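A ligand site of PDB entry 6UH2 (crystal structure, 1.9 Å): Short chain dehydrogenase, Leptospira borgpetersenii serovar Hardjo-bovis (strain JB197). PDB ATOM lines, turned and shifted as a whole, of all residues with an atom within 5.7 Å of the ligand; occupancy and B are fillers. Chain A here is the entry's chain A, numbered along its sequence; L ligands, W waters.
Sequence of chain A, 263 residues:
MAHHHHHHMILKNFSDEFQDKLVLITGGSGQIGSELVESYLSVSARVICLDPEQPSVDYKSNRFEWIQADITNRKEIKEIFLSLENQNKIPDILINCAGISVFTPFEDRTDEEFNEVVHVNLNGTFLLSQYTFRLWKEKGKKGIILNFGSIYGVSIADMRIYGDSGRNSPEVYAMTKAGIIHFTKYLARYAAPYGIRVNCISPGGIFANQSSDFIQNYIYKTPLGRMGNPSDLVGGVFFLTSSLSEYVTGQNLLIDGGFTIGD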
ATOM      1  N   THR A  26       7.956 -15.530   6.209  1.00  0.00           N
ATOM      2  CA  THR A  26       8.551 -14.565   7.124  1.00  0.00           C
ATOM      3  C   THR A  26       7.724 -13.289   7.090  1.00  0.00           C
ATOM      4  O   THR A  26       7.130 -12.937   6.067  1.00  0.00           O
ATOM      5  CB  THR A  26      10.006 -14.237   6.744  1.00  0.00           C
ATOM      6  OG1 THR A  26      10.031 -13.372   5.602  1.00  0.00           O
ATOM      7  CG2 THR A  26      10.785 -15.503   6.439  1.00  0.00           C
ATOM      8  N   GLY A  27       7.662 -12.596   8.227  1.00  0.00           N
ATOM      9  CA  GLY A  27       6.894 -11.369   8.283  1.00  0.00           C
ATOM     10  C   GLY A  27       5.404 -11.575   8.188  1.00  0.00           C
ATOM     11  O   GLY A  27       4.671 -10.660   7.809  1.00  0.00           O
ATOM     12  N   GLY A  28       4.925 -12.772   8.543  1.00  0.00           N
ATOM     13  CA  GLY A  28       3.532 -13.153   8.380  1.00  0.00           C
ATOM     14  C   GLY A  28       2.579 -12.441   9.308  1.00  0.00           C
ATOM     15  O   GLY A  28       1.362 -12.522   9.097  1.00  0.00           O
ATOM     16  N   SER A  29       3.080 -11.717  10.306  1.00  0.00           N
ATOM     17  CA  SER A  29       2.233 -10.941  11.195  1.00  0.00           C
ATOM     18  C   SER A  29       1.896  -9.543  10.670  1.00  0.00           C
ATOM     19  O   SER A  29       1.053  -8.863  11.254  1.00  0.00           O
ATOM     20  CB  SER A  29       2.889 -10.803  12.575  1.00  0.00           C
ATOM     21  OG  SER A  29       3.067 -12.081  13.168  1.00  0.00           O
ATOM     22  N   GLY A  30       2.517  -9.110   9.574  1.00  0.00           N
ATOM     23  CA  GLY A  30       2.364  -7.747   9.110  1.00  0.00           C
ATOM     24  C   GLY A  30       1.127  -7.566   8.245  1.00  0.00           C
ATOM     25  O   GLY A  30       0.270  -8.445   8.146  1.00  0.00           O
ATOM     26  N   GLN A  31       1.044  -6.395   7.602  1.00  0.00           N
ATOM     27  CA  GLN A  31      -0.167  -6.082   6.848  1.00  0.00           C
ATOM     28  C   GLN A  31      -0.352  -7.019   5.663  1.00  0.00           C
ATOM     29  O   GLN A  31      -1.422  -7.629   5.494  1.00  0.00           O
ATOM     30  CB  GLN A  31      -0.164  -4.633   6.379  1.00  0.00           C
ATOM     31  CG  GLN A  31      -1.451  -4.286   5.638  1.00  0.00           C
ATOM     32  CD  GLN A  31      -1.560  -2.832   5.273  1.00  0.00           C
ATOM     33  OE1 GLN A  31      -0.544  -2.114   5.235  1.00  0.00           O
ATOM     34  NE2 GLN A  31      -2.787  -2.371   5.018  1.00  0.00           N
ATOM     35  N   ILE A  32       0.673  -7.171   4.822  1.00  0.00           N
ATOM     36  CA  ILE A  32       0.559  -8.086   3.685  1.00  0.00           C
ATOM     37  C   ILE A  32       0.645  -9.527   4.149  1.00  0.00           C
ATOM     38  O   ILE A  32      -0.111 -10.385   3.683  1.00  0.00           O
ATOM     39  CB  ILE A  32       1.640  -7.783   2.633  1.00  0.00           C
ATOM     40  CG1 ILE A  32       1.418  -6.404   2.003  1.00  0.00           C
ATOM     41  CG2 ILE A  32       1.648  -8.889   1.558  1.00  0.00           C
ATOM     42  CD1 ILE A  32       2.619  -5.935   1.187  1.00  0.00           C
ATOM     43  N   GLY A  33       1.566  -9.801   5.074  1.00  0.00           N
ATOM     44  CA  GLY A  33       1.796 -11.176   5.515  1.00  0.00           C
ATOM     45  C   GLY A  33       0.562 -11.826   6.099  1.00  0.00           C
ATOM     46  O   GLY A  33       0.283 -12.982   5.828  1.00  0.00           O
ATOM     47  N   LEU A  50       7.002 -16.872  10.568  1.00  0.00           N
ATOM     48  CA  LEU A  50       8.189 -16.448  11.313  1.00  0.00           C
ATOM     49  C   LEU A  50       8.142 -14.930  11.440  1.00  0.00           C
ATOM     50  O   LEU A  50       8.187 -14.216  10.428  1.00  0.00           O
ATOM     51  CB  LEU A  50       9.491 -16.860  10.625  1.00  0.00           C
ATOM     52  CG  LEU A  50       9.802 -18.324  10.370  1.00  0.00           C
ATOM     53  CD1 LEU A  50      11.173 -18.425   9.713  1.00  0.00           C
ATOM     54  CD2 LEU A  50       9.780 -19.108  11.659  1.00  0.00           C
ATOM     55  N   ASP A  51       8.081 -14.444  12.677  1.00  0.00           N
ATOM     56  CA  ASP A  51       7.898 -13.025  12.928  1.00  0.00           C
ATOM     57  C   ASP A  51       8.226 -12.777  14.392  1.00  0.00           C
ATOM     58  O   ASP A  51       7.845 -13.567  15.255  1.00  0.00           O
ATOM     59  CB  ASP A  51       6.460 -12.601  12.596  1.00  0.00           C
ATOM     60  CG  ASP A  51       6.330 -11.124  12.263  1.00  0.00           C
ATOM     61  OD1 ASP A  51       6.736 -10.265  13.096  1.00  0.00           O
ATOM     62  OD2 ASP A  51       5.792 -10.803  11.179  1.00  0.00           O
ATOM     63  N   PRO A  52       8.966 -11.710  14.721  1.00  0.00           N
ATOM     64  CA  PRO A  52       9.153 -11.404  16.141  1.00  0.00           C
ATOM     65  C   PRO A  52       7.876 -10.952  16.812  1.00  0.00           C
ATOM     66  O   PRO A  52       7.815 -10.960  18.047  1.00  0.00           O
ATOM     67  CB  PRO A  52      10.217 -10.299  16.129  1.00  0.00           C
ATOM     68  CG  PRO A  52      10.083  -9.665  14.783  1.00  0.00           C
ATOM     69  CD  PRO A  52       9.703 -10.780  13.850  1.00  0.00           C
ATOM     70  N   GLU A  53       6.857 -10.584  16.035  1.00  0.00           N
ATOM     71  CA  GLU A  53       5.590 -10.075  16.543  1.00  0.00           C
ATOM     72  C   GLU A  53       4.510 -11.140  16.457  1.00  0.00           C
ATOM     73  O   GLU A  53       4.384 -11.829  15.444  1.00  0.00           O
ATOM     74  CB  GLU A  53       5.145  -8.850  15.732  1.00  0.00           C
ATOM     75  CG  GLU A  53       5.921  -7.593  16.009  1.00  0.00           C
ATOM     76  CD  GLU A  53       5.604  -7.026  17.383  1.00  0.00           C
ATOM     77  OE1 GLU A  53       4.505  -7.320  17.910  1.00  0.00           O
ATOM     78  OE2 GLU A  53       6.451  -6.292  17.931  1.00  0.00           O
ATOM     79  N   ALA A  69      10.498 -15.377  15.850  1.00  0.00           N
ATOM     80  CA  ALA A  69      11.855 -15.499  15.339  1.00  0.00           C
ATOM     81  C   ALA A  69      12.285 -14.213  14.653  1.00  0.00           C
ATOM     82  O   ALA A  69      11.455 -13.447  14.138  1.00  0.00           O
ATOM     83  CB  ALA A  69      11.984 -16.672  14.370  1.00  0.00           C
ATOM     84  N   ASP A  70      13.602 -14.007  14.625  1.00  0.00           N
ATOM     85  CA  ASP A  70      14.239 -12.842  14.026  1.00  0.00           C
ATOM     86  C   ASP A  70      15.098 -13.356  12.883  1.00  0.00           C
ATOM     87  O   ASP A  70      16.113 -14.033  13.110  1.00  0.00           O
ATOM     88  CB  ASP A  70      15.056 -12.099  15.088  1.00  0.00           C
ATOM     89  CG  ASP A  70      15.922 -10.992  14.538  1.00  0.00           C
ATOM     90  OD1 ASP A  70      15.872 -10.682  13.323  1.00  0.00           O
ATOM     91  OD2 ASP A  70      16.659 -10.409  15.348  1.00  0.00           O
ATOM     92  N   ILE A  71      14.699 -13.059  11.641  1.00  0.00           N
ATOM     93  CA  ILE A  71      15.388 -13.614  10.480  1.00  0.00           C
ATOM     94  C   ILE A  71      16.773 -13.034  10.262  1.00  0.00           C
ATOM     95  O   ILE A  71      17.513 -13.545   9.410  1.00  0.00           O
ATOM     96  CB  ILE A  71      14.588 -13.438   9.179  1.00  0.00           C
ATOM     97  CG1 ILE A  71      14.476 -11.960   8.795  1.00  0.00           C
ATOM     98  CG2 ILE A  71      13.244 -14.123   9.294  1.00  0.00           C
ATOM     99  CD1 ILE A  71      13.566 -11.706   7.591  1.00  0.00           C
ATOM    100  N   THR A  72      17.146 -11.985  10.984  1.00  0.00           N
ATOM    101  CA  THR A  72      18.525 -11.509  10.901  1.00  0.00           C
ATOM    102  C   THR A  72      19.475 -12.337  11.763  1.00  0.00           C
ATOM    103  O   THR A  72      20.688 -12.110  11.716  1.00  0.00           O
ATOM    104  CB  THR A  72      18.629 -10.027  11.308  1.00  0.00           C
ATOM    105  OG1 THR A  72      18.456  -9.884  12.736  1.00  0.00           O
ATOM    106  CG2 THR A  72      17.582  -9.197  10.586  1.00  0.00           C
ATOM    107  N   ASN A  96       9.304 -14.842   1.361  1.00  0.00           N
ATOM    108  CA  ASN A  96      10.174 -13.908   2.091  1.00  0.00           C
ATOM    109  C   ASN A  96       9.474 -12.562   2.108  1.00  0.00           C
ATOM    110  O   ASN A  96       9.778 -11.656   1.343  1.00  0.00           O
ATOM    111  CB  ASN A  96      11.554 -13.810   1.449  1.00  0.00           C
ATOM    112  CG  ASN A  96      12.428 -15.029   1.730  1.00  0.00           C
ATOM    113  OD1 ASN A  96      12.630 -15.412   2.895  1.00  0.00           O
ATOM    114  ND2 ASN A  96      12.933 -15.655   0.662  1.00  0.00           N
ATOM    115  N   CYS A  97       8.489 -12.456   2.994  1.00  0.00           N
ATOM    116  CA  CYS A  97       7.660 -11.261   3.041  1.00  0.00           C
ATOM    117  C   CYS A  97       8.220 -10.202   3.979  1.00  0.00           C
ATOM    118  O   CYS A  97       7.947  -9.019   3.778  1.00  0.00           O
ATOM    119  CB  CYS A  97       6.221 -11.634   3.443  1.00  0.00           C
ATOM    120  SG  CYS A  97       4.968 -10.353   3.089  1.00  0.00           S
ATOM    121  N   ALA A  98       9.021 -10.588   4.967  1.00  0.00           N
ATOM    122  CA  ALA A  98       9.513  -9.611   5.938  1.00  0.00           C
ATOM    123  C   ALA A  98      10.312  -8.512   5.241  1.00  0.00           C
ATOM    124  O   ALA A  98      11.157  -8.786   4.389  1.00  0.00           O
ATOM    125  CB  ALA A  98      10.385 -10.304   6.976  1.00  0.00           C
ATOM    126  N   GLY A  99      10.066  -7.268   5.634  1.00  0.00           N
ATOM    127  CA  GLY A  99      10.825  -6.134   5.133  1.00  0.00           C
ATOM    128  C   GLY A  99      10.555  -4.922   5.980  1.00  0.00           C
ATOM    129  O   GLY A  99       9.483  -4.810   6.598  1.00  0.00           O
ATOM    130  N   ILE A 100      11.531  -4.013   6.041  1.00  0.00           N
ATOM    131  CA  ILE A 100      11.415  -2.769   6.804  1.00  0.00           C
ATOM    132  C   ILE A 100      12.002  -1.612   6.007  1.00  0.00           C
ATOM    133  O   ILE A 100      12.640  -1.787   4.968  1.00  0.00           O
ATOM    134  CB  ILE A 100      12.101  -2.844   8.185  1.00  0.00           C
ATOM    135  CG1 ILE A 100      13.621  -2.987   8.006  1.00  0.00           C
ATOM    136  CG2 ILE A 100      11.525  -3.985   9.034  1.00  0.00           C
ATOM    137  CD1 ILE A 100      14.410  -2.781   9.282  1.00  0.00           C
ATOM    138  N   VAL A 120      17.415  -6.870   7.643  1.00  0.00           N
ATOM    139  CA  VAL A 120      16.108  -7.494   7.476  1.00  0.00           C
ATOM    140  C   VAL A 120      15.861  -7.828   6.013  1.00  0.00           C
ATOM    141  O   VAL A 120      15.496  -8.961   5.671  1.00  0.00           O
ATOM    142  CB  VAL A 120      14.994  -6.592   8.042  1.00  0.00           C
ATOM    143  CG1 VAL A 120      13.636  -7.227   7.764  1.00  0.00           C
ATOM    144  CG2 VAL A 120      15.192  -6.367   9.538  1.00  0.00           C
ATOM    145  N   ASN A 121      16.084  -6.863   5.124  1.00  0.00           N
ATOM    146  CA  ASN A 121      15.690  -7.024   3.717  1.00  0.00           C
ATOM    147  C   ASN A 121      16.663  -7.928   2.960  1.00  0.00           C
ATOM    148  O   ASN A 121      16.239  -8.847   2.249  1.00  0.00           O
ATOM    149  CB  ASN A 121      15.596  -5.650   3.043  1.00  0.00           C
ATOM    150  CG  ASN A 121      14.491  -4.786   3.635  1.00  0.00           C
ATOM    151  OD1 ASN A 121      13.865  -5.149   4.631  1.00  0.00           O
ATOM    152  ND2 ASN A 121      14.293  -3.605   3.053  1.00  0.00           N
ATOM    153  N   PHE A 148       9.738 -10.659  -1.918  1.00  0.00           N
ATOM    154  CA  PHE A 148       8.973  -9.427  -2.003  1.00  0.00           C
ATOM    155  C   PHE A 148       9.906  -8.266  -2.315  1.00  0.00           C
ATOM    156  O   PHE A 148      10.820  -7.972  -1.531  1.00  0.00           O
ATOM    157  CB  PHE A 148       8.163  -9.185  -0.722  1.00  0.00           C
ATOM    158  CG  PHE A 148       6.773  -9.704  -0.812  1.00  0.00           C
ATOM    159  CD1 PHE A 148       6.519 -11.077  -0.775  1.00  0.00           C
ATOM    160  CD2 PHE A 148       5.711  -8.835  -1.012  1.00  0.00           C
ATOM    161  CE1 PHE A 148       5.221 -11.560  -0.912  1.00  0.00           C
ATOM    162  CE2 PHE A 148       4.422  -9.311  -1.141  1.00  0.00           C
ATOM    163  CZ  PHE A 148       4.173 -10.685  -1.096  1.00  0.00           C
ATOM    164  N   GLY A 149       9.714  -7.661  -3.475  1.00  0.00           N
ATOM    165  CA  GLY A 149      10.444  -6.458  -3.816  1.00  0.00           C
ATOM    166  C   GLY A 149       9.620  -5.246  -3.454  1.00  0.00           C
ATOM    167  O   GLY A 149       9.048  -5.187  -2.366  1.00  0.00           O
ATOM    168  N   SER A 150       9.546  -4.283  -4.370  1.00  0.00           N
ATOM    169  CA  SER A 150       8.819  -3.036  -4.209  1.00  0.00           C
ATOM    170  C   SER A 150       8.903  -2.293  -5.528  1.00  0.00           C
ATOM    171  O   SER A 150       9.868  -2.468  -6.281  1.00  0.00           O
ATOM    172  CB  SER A 150       9.390  -2.172  -3.085  1.00  0.00           C
ATOM    173  OG  SER A 150       8.933  -0.827  -3.172  1.00  0.00           O
ATOM    174  N   ILE A 151       7.899  -1.454  -5.788  1.00  0.00           N
ATOM    175  CA  ILE A 151       8.020  -0.485  -6.885  1.00  0.00           C
ATOM    176  C   ILE A 151       9.290   0.338  -6.738  1.00  0.00           C
ATOM    177  O   ILE A 151       9.871   0.784  -7.739  1.00  0.00           O
ATOM    178  CB  ILE A 151       6.763   0.416  -6.967  1.00  0.00           C
ATOM    179  CG1 ILE A 151       6.424   1.034  -5.610  1.00  0.00           C
ATOM    180  CG2 ILE A 151       5.601  -0.370  -7.494  1.00  0.00           C
ATOM    181  CD1 ILE A 151       5.495   2.218  -5.718  1.00  0.00           C
ATOM    182  N   TYR A 173      16.385   1.565   1.146  1.00  0.00           N
ATOM    183  CA  TYR A 173      15.250   0.754   0.714  1.00  0.00           C
ATOM    184  C   TYR A 173      15.329   0.475  -0.784  1.00  0.00           C
ATOM    185  O   TYR A 173      15.119  -0.659  -1.235  1.00  0.00           O
ATOM    186  CB  TYR A 173      13.946   1.455   1.102  1.00  0.00           C
ATOM    187  CG  TYR A 173      12.716   0.586   0.945  1.00  0.00           C
ATOM    188  CD1 TYR A 173      12.411  -0.411   1.866  1.00  0.00           C
ATOM    189  CD2 TYR A 173      11.875   0.753  -0.144  1.00  0.00           C
ATOM    190  CE1 TYR A 173      11.283  -1.215   1.715  1.00  0.00           C
ATOM    191  CE2 TYR A 173      10.752  -0.047  -0.318  1.00  0.00           C
ATOM    192  CZ  TYR A 173      10.452  -1.018   0.625  1.00  0.00           C
ATOM    193  OH  TYR A 173       9.339  -1.811   0.458  1.00  0.00           O
ATOM    194  N   LYS A 177      15.779  -3.320  -2.065  1.00  0.00           N
ATOM    195  CA  LYS A 177      14.738  -3.926  -2.910  1.00  0.00           C
ATOM    196  C   LYS A 177      15.255  -4.220  -4.323  1.00  0.00           C
ATOM    197  O   LYS A 177      14.932  -5.262  -4.903  1.00  0.00           O
ATOM    198  CB  LYS A 177      13.489  -3.026  -2.919  1.00  0.00           C
ATOM    199  CG  LYS A 177      12.745  -3.058  -1.571  1.00  0.00           C
ATOM    200  CD  LYS A 177      12.394  -4.498  -1.139  1.00  0.00           C
ATOM    201  CE  LYS A 177      11.522  -4.526   0.144  1.00  0.00           C
ATOM    202  NZ  LYS A 177      11.058  -5.891   0.532  1.00  0.00           N
ATOM    203  N   SER A 202       6.642  -7.335  -6.611  1.00  0.00           N
ATOM    204  CA  SER A 202       6.921  -5.973  -6.158  1.00  0.00           C
ATOM    205  C   SER A 202       5.608  -5.211  -6.032  1.00  0.00           C
ATOM    206  O   SER A 202       5.041  -4.750  -7.047  1.00  0.00           O
ATOM    207  CB  SER A 202       7.868  -5.276  -7.139  1.00  0.00           C
ATOM    208  OG  SER A 202       9.117  -5.947  -7.185  1.00  0.00           O
ATOM    209  N   PRO A 203       5.070  -5.049  -4.830  1.00  0.00           N
ATOM    210  CA  PRO A 203       3.824  -4.282  -4.689  1.00  0.00           C
ATOM    211  C   PRO A 203       4.051  -2.808  -4.923  1.00  0.00           C
ATOM    212  O   PRO A 203       5.132  -2.260  -4.655  1.00  0.00           O
ATOM    213  CB  PRO A 203       3.396  -4.551  -3.235  1.00  0.00           C
ATOM    214  CG  PRO A 203       4.210  -5.766  -2.798  1.00  0.00           C
ATOM    215  CD  PRO A 203       5.512  -5.611  -3.554  1.00  0.00           C
ATOM    216  N   GLY A 204       3.001  -2.155  -5.431  1.00  0.00           N
ATOM    217  CA  GLY A 204       2.911  -0.724  -5.327  1.00  0.00           C
ATOM    218  C   GLY A 204       2.498  -0.332  -3.928  1.00  0.00           C
ATOM    219  O   GLY A 204       2.340  -1.169  -3.044  1.00  0.00           O
ATOM    220  N   GLY A 205       2.328   0.965  -3.726  1.00  0.00           N
ATOM    221  CA  GLY A 205       1.914   1.484  -2.434  1.00  0.00           C
ATOM    222  C   GLY A 205       0.653   0.818  -1.906  1.00  0.00           C
ATOM    223  O   GLY A 205      -0.364   0.746  -2.603  1.00  0.00           O
ATOM    224  N   ILE A 206       0.721   0.294  -0.685  1.00  0.00           N
ATOM    225  CA  ILE A 206      -0.428  -0.328  -0.036  1.00  0.00           C
ATOM    226  C   ILE A 206      -1.000   0.673   0.963  1.00  0.00           C
ATOM    227  O   ILE A 206      -0.256   1.250   1.769  1.00  0.00           O
ATOM    228  CB  ILE A 206      -0.024  -1.635   0.664  1.00  0.00           C
ATOM    229  CG1 ILE A 206       0.602  -2.616  -0.345  1.00  0.00           C
ATOM    230  CG2 ILE A 206      -1.220  -2.261   1.365  1.00  0.00           C
ATOM    231  CD1 ILE A 206      -0.348  -3.117  -1.438  1.00  0.00           C
ATOM    232  N   PHE A 207      -2.309   0.873   0.904  1.00  0.00           N
ATOM    233  CA  PHE A 207      -2.962   1.782   1.842  1.00  0.00           C
ATOM    234  C   PHE A 207      -2.764   1.271   3.271  1.00  0.00           C
ATOM    235  O   PHE A 207      -3.120   0.139   3.591  1.00  0.00           O
ATOM    236  CB  PHE A 207      -4.448   1.900   1.514  1.00  0.00           C
ATOM    237  CG  PHE A 207      -5.219   2.743   2.496  1.00  0.00           C
ATOM    238  CD1 PHE A 207      -4.841   4.052   2.761  1.00  0.00           C
ATOM    239  CD2 PHE A 207      -6.320   2.230   3.167  1.00  0.00           C
ATOM    240  CE1 PHE A 207      -5.539   4.824   3.673  1.00  0.00           C
ATOM    241  CE2 PHE A 207      -7.028   2.995   4.072  1.00  0.00           C
ATOM    242  CZ  PHE A 207      -6.630   4.300   4.327  1.00  0.00           C
ATOM    243  N   GLN A 210      -0.975   6.446   5.820  1.00  0.00           N
ATOM    244  CA  GLN A 210      -0.408   7.571   5.094  1.00  0.00           C
ATOM    245  C   GLN A 210      -1.368   8.753   5.097  1.00  0.00           C
ATOM    246  O   GLN A 210      -2.589   8.581   5.087  1.00  0.00           O
ATOM    247  CB  GLN A 210      -0.074   7.178   3.652  1.00  0.00           C
ATOM    248  CG  GLN A 210       0.835   5.967   3.515  1.00  0.00           C
ATOM    249  CD  GLN A 210       0.078   4.697   3.186  1.00  0.00           C
ATOM    250  OE1 GLN A 210      -1.141   4.612   3.400  1.00  0.00           O
ATOM    251  NE2 GLN A 210       0.783   3.703   2.664  1.00  0.00           N
HETATM  252  P1  LIG L   1       4.571  -4.509   7.772  1.00  0.00           P
HETATM  253  O1  LIG L   1       5.537  -3.517   8.456  1.00  0.00           O
HETATM  254  O2  LIG L   1       3.038  -4.468   7.958  1.00  0.00           O
HETATM  255  O3  LIG L   1       5.083  -6.039   8.058  1.00  0.00           O
HETATM  256  C1  LIG L   1       6.451  -6.379   8.079  1.00  0.00           C
HETATM  257  C2  LIG L   1       6.502  -7.585   8.971  1.00  0.00           C
HETATM  258  O4  LIG L   1       7.915  -7.989   8.967  1.00  0.00           O
HETATM  259  C3  LIG L   1       6.127  -7.270  10.434  1.00  0.00           C
HETATM  260  O5  LIG L   1       5.237  -8.294  10.936  1.00  0.00           O
HETATM  261  C4  LIG L   1       7.468  -7.382  11.163  1.00  0.00           C
HETATM  262  O6  LIG L   1       7.288  -7.849  12.494  1.00  0.00           O
HETATM  263  C5  LIG L   1       8.230  -8.387  10.268  1.00  0.00           C
HETATM  264  N1  LIG L   1       9.656  -8.278  10.567  1.00  0.00           N
HETATM  265  C6  LIG L   1      10.409  -7.135  10.767  1.00  0.00           C
HETATM  266  N2  LIG L   1      11.638  -7.423  11.069  1.00  0.00           N
HETATM  267  C7  LIG L   1      11.707  -8.809  11.098  1.00  0.00           C
HETATM  268  C8  LIG L   1      12.736  -9.713  11.374  1.00  0.00           C
HETATM  269  N3  LIG L   1      13.964  -9.315  11.685  1.00  0.00           N
HETATM  270  N4  LIG L   1      12.460 -11.017  11.306  1.00  0.00           N
HETATM  271  C9  LIG L   1      11.233 -11.428  10.994  1.00  0.00           C
HETATM  272  N5  LIG L   1      10.194 -10.655  10.721  1.00  0.00           N
HETATM  273  C10 LIG L   1      10.475  -9.343  10.787  1.00  0.00           C
HETATM  274  O7  LIG L   1       4.854  -4.520   6.168  1.00  0.00           O
HETATM  275  P2  LIG L   1       3.987  -4.938   4.874  1.00  0.00           P
HETATM  276  O8  LIG L   1       3.376  -3.701   4.189  1.00  0.00           O
HETATM  277  O9  LIG L   1       3.159  -6.171   5.210  1.00  0.00           O
HETATM  278  O10 LIG L   1       5.256  -5.364   3.838  1.00  0.00           O
HETATM  279  C11 LIG L   1       5.503  -6.719   3.522  1.00  0.00           C
HETATM  280  C12 LIG L   1       6.531  -6.733   2.398  1.00  0.00           C
HETATM  281  O11 LIG L   1       6.090  -5.902   1.255  1.00  0.00           O
HETATM  282  C13 LIG L   1       7.826  -6.053   2.837  1.00  0.00           C
HETATM  283  O12 LIG L   1       8.973  -6.678   2.206  1.00  0.00           O
HETATM  284  C14 LIG L   1       7.741  -4.589   2.309  1.00  0.00           C
HETATM  285  O13 LIG L   1       9.014  -4.049   2.048  1.00  0.00           O
HETATM  286  C15 LIG L   1       6.980  -4.865   0.983  1.00  0.00           C
HETATM  287  N6  LIG L   1       6.206  -3.699   0.404  1.00  0.00           N
HETATM  288  C16 LIG L   1       5.234  -3.051   1.094  1.00  0.00           C
HETATM  289  C17 LIG L   1       4.565  -2.003   0.504  1.00  0.00           C
HETATM  290  C18 LIG L   1       3.512  -1.297   1.299  1.00  0.00           C
HETATM  291  O14 LIG L   1       3.068  -0.224   0.888  1.00  0.00           O
HETATM  292  N7  LIG L   1       3.093  -1.855   2.450  1.00  0.00           N
HETATM  293  C19 LIG L   1       4.917  -1.632  -0.800  1.00  0.00           C
HETATM  294  C20 LIG L   1       5.889  -2.302  -1.481  1.00  0.00           C
HETATM  295  C21 LIG L   1       6.530  -3.358  -0.847  1.00  0.00           C
HETATM  296  O   HOH W   1      12.981  -5.699  12.827  1.00  0.00           O
HETATM  297  O   HOH W   2       8.126  -3.095   8.072  1.00  0.00           O
HETATM  298  O   HOH W   3       1.638  -2.014   7.893  1.00  0.00           O
HETATM  299  O   HOH W   4       3.580  -6.936  12.811  1.00  0.00           O
HETATM  300  O   HOH W   5       1.757   0.382   3.440  1.00  0.00           O
HETATM  301  O   HOH W   6       8.727  -4.174  11.185  1.00  0.00           O
HETATM  302  O   HOH W   7       3.767  -8.354   6.125  1.00  0.00           O
HETATM  303  O   HOH W   8      15.312  -6.773  12.818  1.00  0.00           O
HETATM  304  O   HOH W   9      12.182  -7.805   1.875  1.00  0.00           O
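The side-chain carboxylate of Asp 51 is in hydrogen-bond range of an oxygen (O6) of the ligand (2.6 Å). The backbone NH (N) of Ile 32 sits at hydrogen-bond distance from an oxygen (O9) of the ligand (2.7 Å). The side-chain hydroxyl (OH) of Tyr 173 is in hydrogen-bond range of an oxygen (O13) of the ligand (2.8 Å). NZ of Lys 177 lies within hydrogen-bond range of O12 of the ligand, 2.8 Å away. The backbone NH (N) of Gln 31 sits at hydrogen-bond distance from an oxygen (O2) of the ligand (2.8 Å). The side-chain carboxylate (OD1) of Asp 70 sits at hydrogen-bond distance from a nitrogen (N3) of the ligand (2.9 Å). O14 of the ligand lies within hydrogen-bond range of N of Ile 206 (2.9 Å). The backbone carbonyl oxygen of Cys 97 lies within hydrogen-bond range of an oxygen (O12) of the ligand, at 3.0 Å. The backbone NH of Ile 71 lies within hydrogen-bond range of a nitrogen (N4) of the ligand. The backbone NH of Gly 30 sits at hydrogen-bond distance from an oxygen (O5) of the ligand (3.1 Å).
The backbone carbonyl oxygen of Asp 51 lies within hydrogen-bond range of the backbone NH of Ala 69, 3.3 Å away. OD1 of Asp 51 sits at hydrogen-bond distance from N of Glu 53 (3.0 Å). The backbone NH of Gly 28 lies within hydrogen-bond range of the side-chain carboxylate of Asp 51 (3.4 Å). NZ of Lys 177 sits at hydrogen-bond distance from O of Phe 148 (2.9 Å). OD1 of Asp 70 lies within hydrogen-bond range of OG1 of Thr 72, at 2.8 Å. The backbone carbonyl oxygen (O) of Ile 206 sits at hydrogen-bond distance from the side-chain amide nitrogen (NE2) of Gln 210 (2.8 Å). OG of Ser 29 sits at hydrogen-bond distance from O of Glu 53, 2.6 Å away. OG1 of Thr 26 is in hydrogen-bond range of N of Ala 98 (3.0 Å).
Residues that only touch the ligand: Gly 27 (3.6 Å), Ser 29 (3.6 Å), Gly 33 (3.97 Å), Pro 52 (3.2 Å), Glu 53 (3.8 Å), Ala 69 (3.7 Å), Thr 72 (3.8 Å), Ala 98 (3.7 Å), Gly 99 (3.5 Å), Ile 100 (3.8 Å), Val 120 (3.8 Å), Phe 148 (3.7 Å), Gly 149 (3.5 Å), Ser 150 (3.8 Å), Pro 203 (3.3 Å), Gly 204 (3.4 Å) and Gly 205 (3.8 Å). Hydrophobic or aromatic side chains that line the ligand: Ile 32, Pro 52, Ile 71, Ala 98, Ile 100, Val 120, Phe 148, Tyr 173, Pro 203 and Ile 206. The nearest printed residue that does not touch the ligand is Leu 50 (4.1 Å).
Water W7 lies within hydrogen-bond range of O9 of the ligand (2.4 Å), N of Gly 33 (2.8 Å) and O of Gly 27 (3.0 Å). Water W2 lies within hydrogen-bond range of O of Gly 99 (2.6 Å) and O1 of the ligand (2.7 Å). Water W5 lies within hydrogen-bond range of the backbone carbonyl oxygen (O) of Ile 206 (2.8 Å) and a nitrogen (N7) of the ligand (2.8 Å). Water W3 lies within hydrogen-bond range of an oxygen (O2) of the ligand (2.8 Å) and the side-chain amide oxygen (OE1) of Gln 31 (3.4 Å). Water W9 lies within hydrogen-bond range of the side-chain amino group of Lys 177 (2.6 Å), the backbone carbonyl oxygen of Ala 98 (2.9 Å) and an oxygen (O12) of the ligand (3.4 Å).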
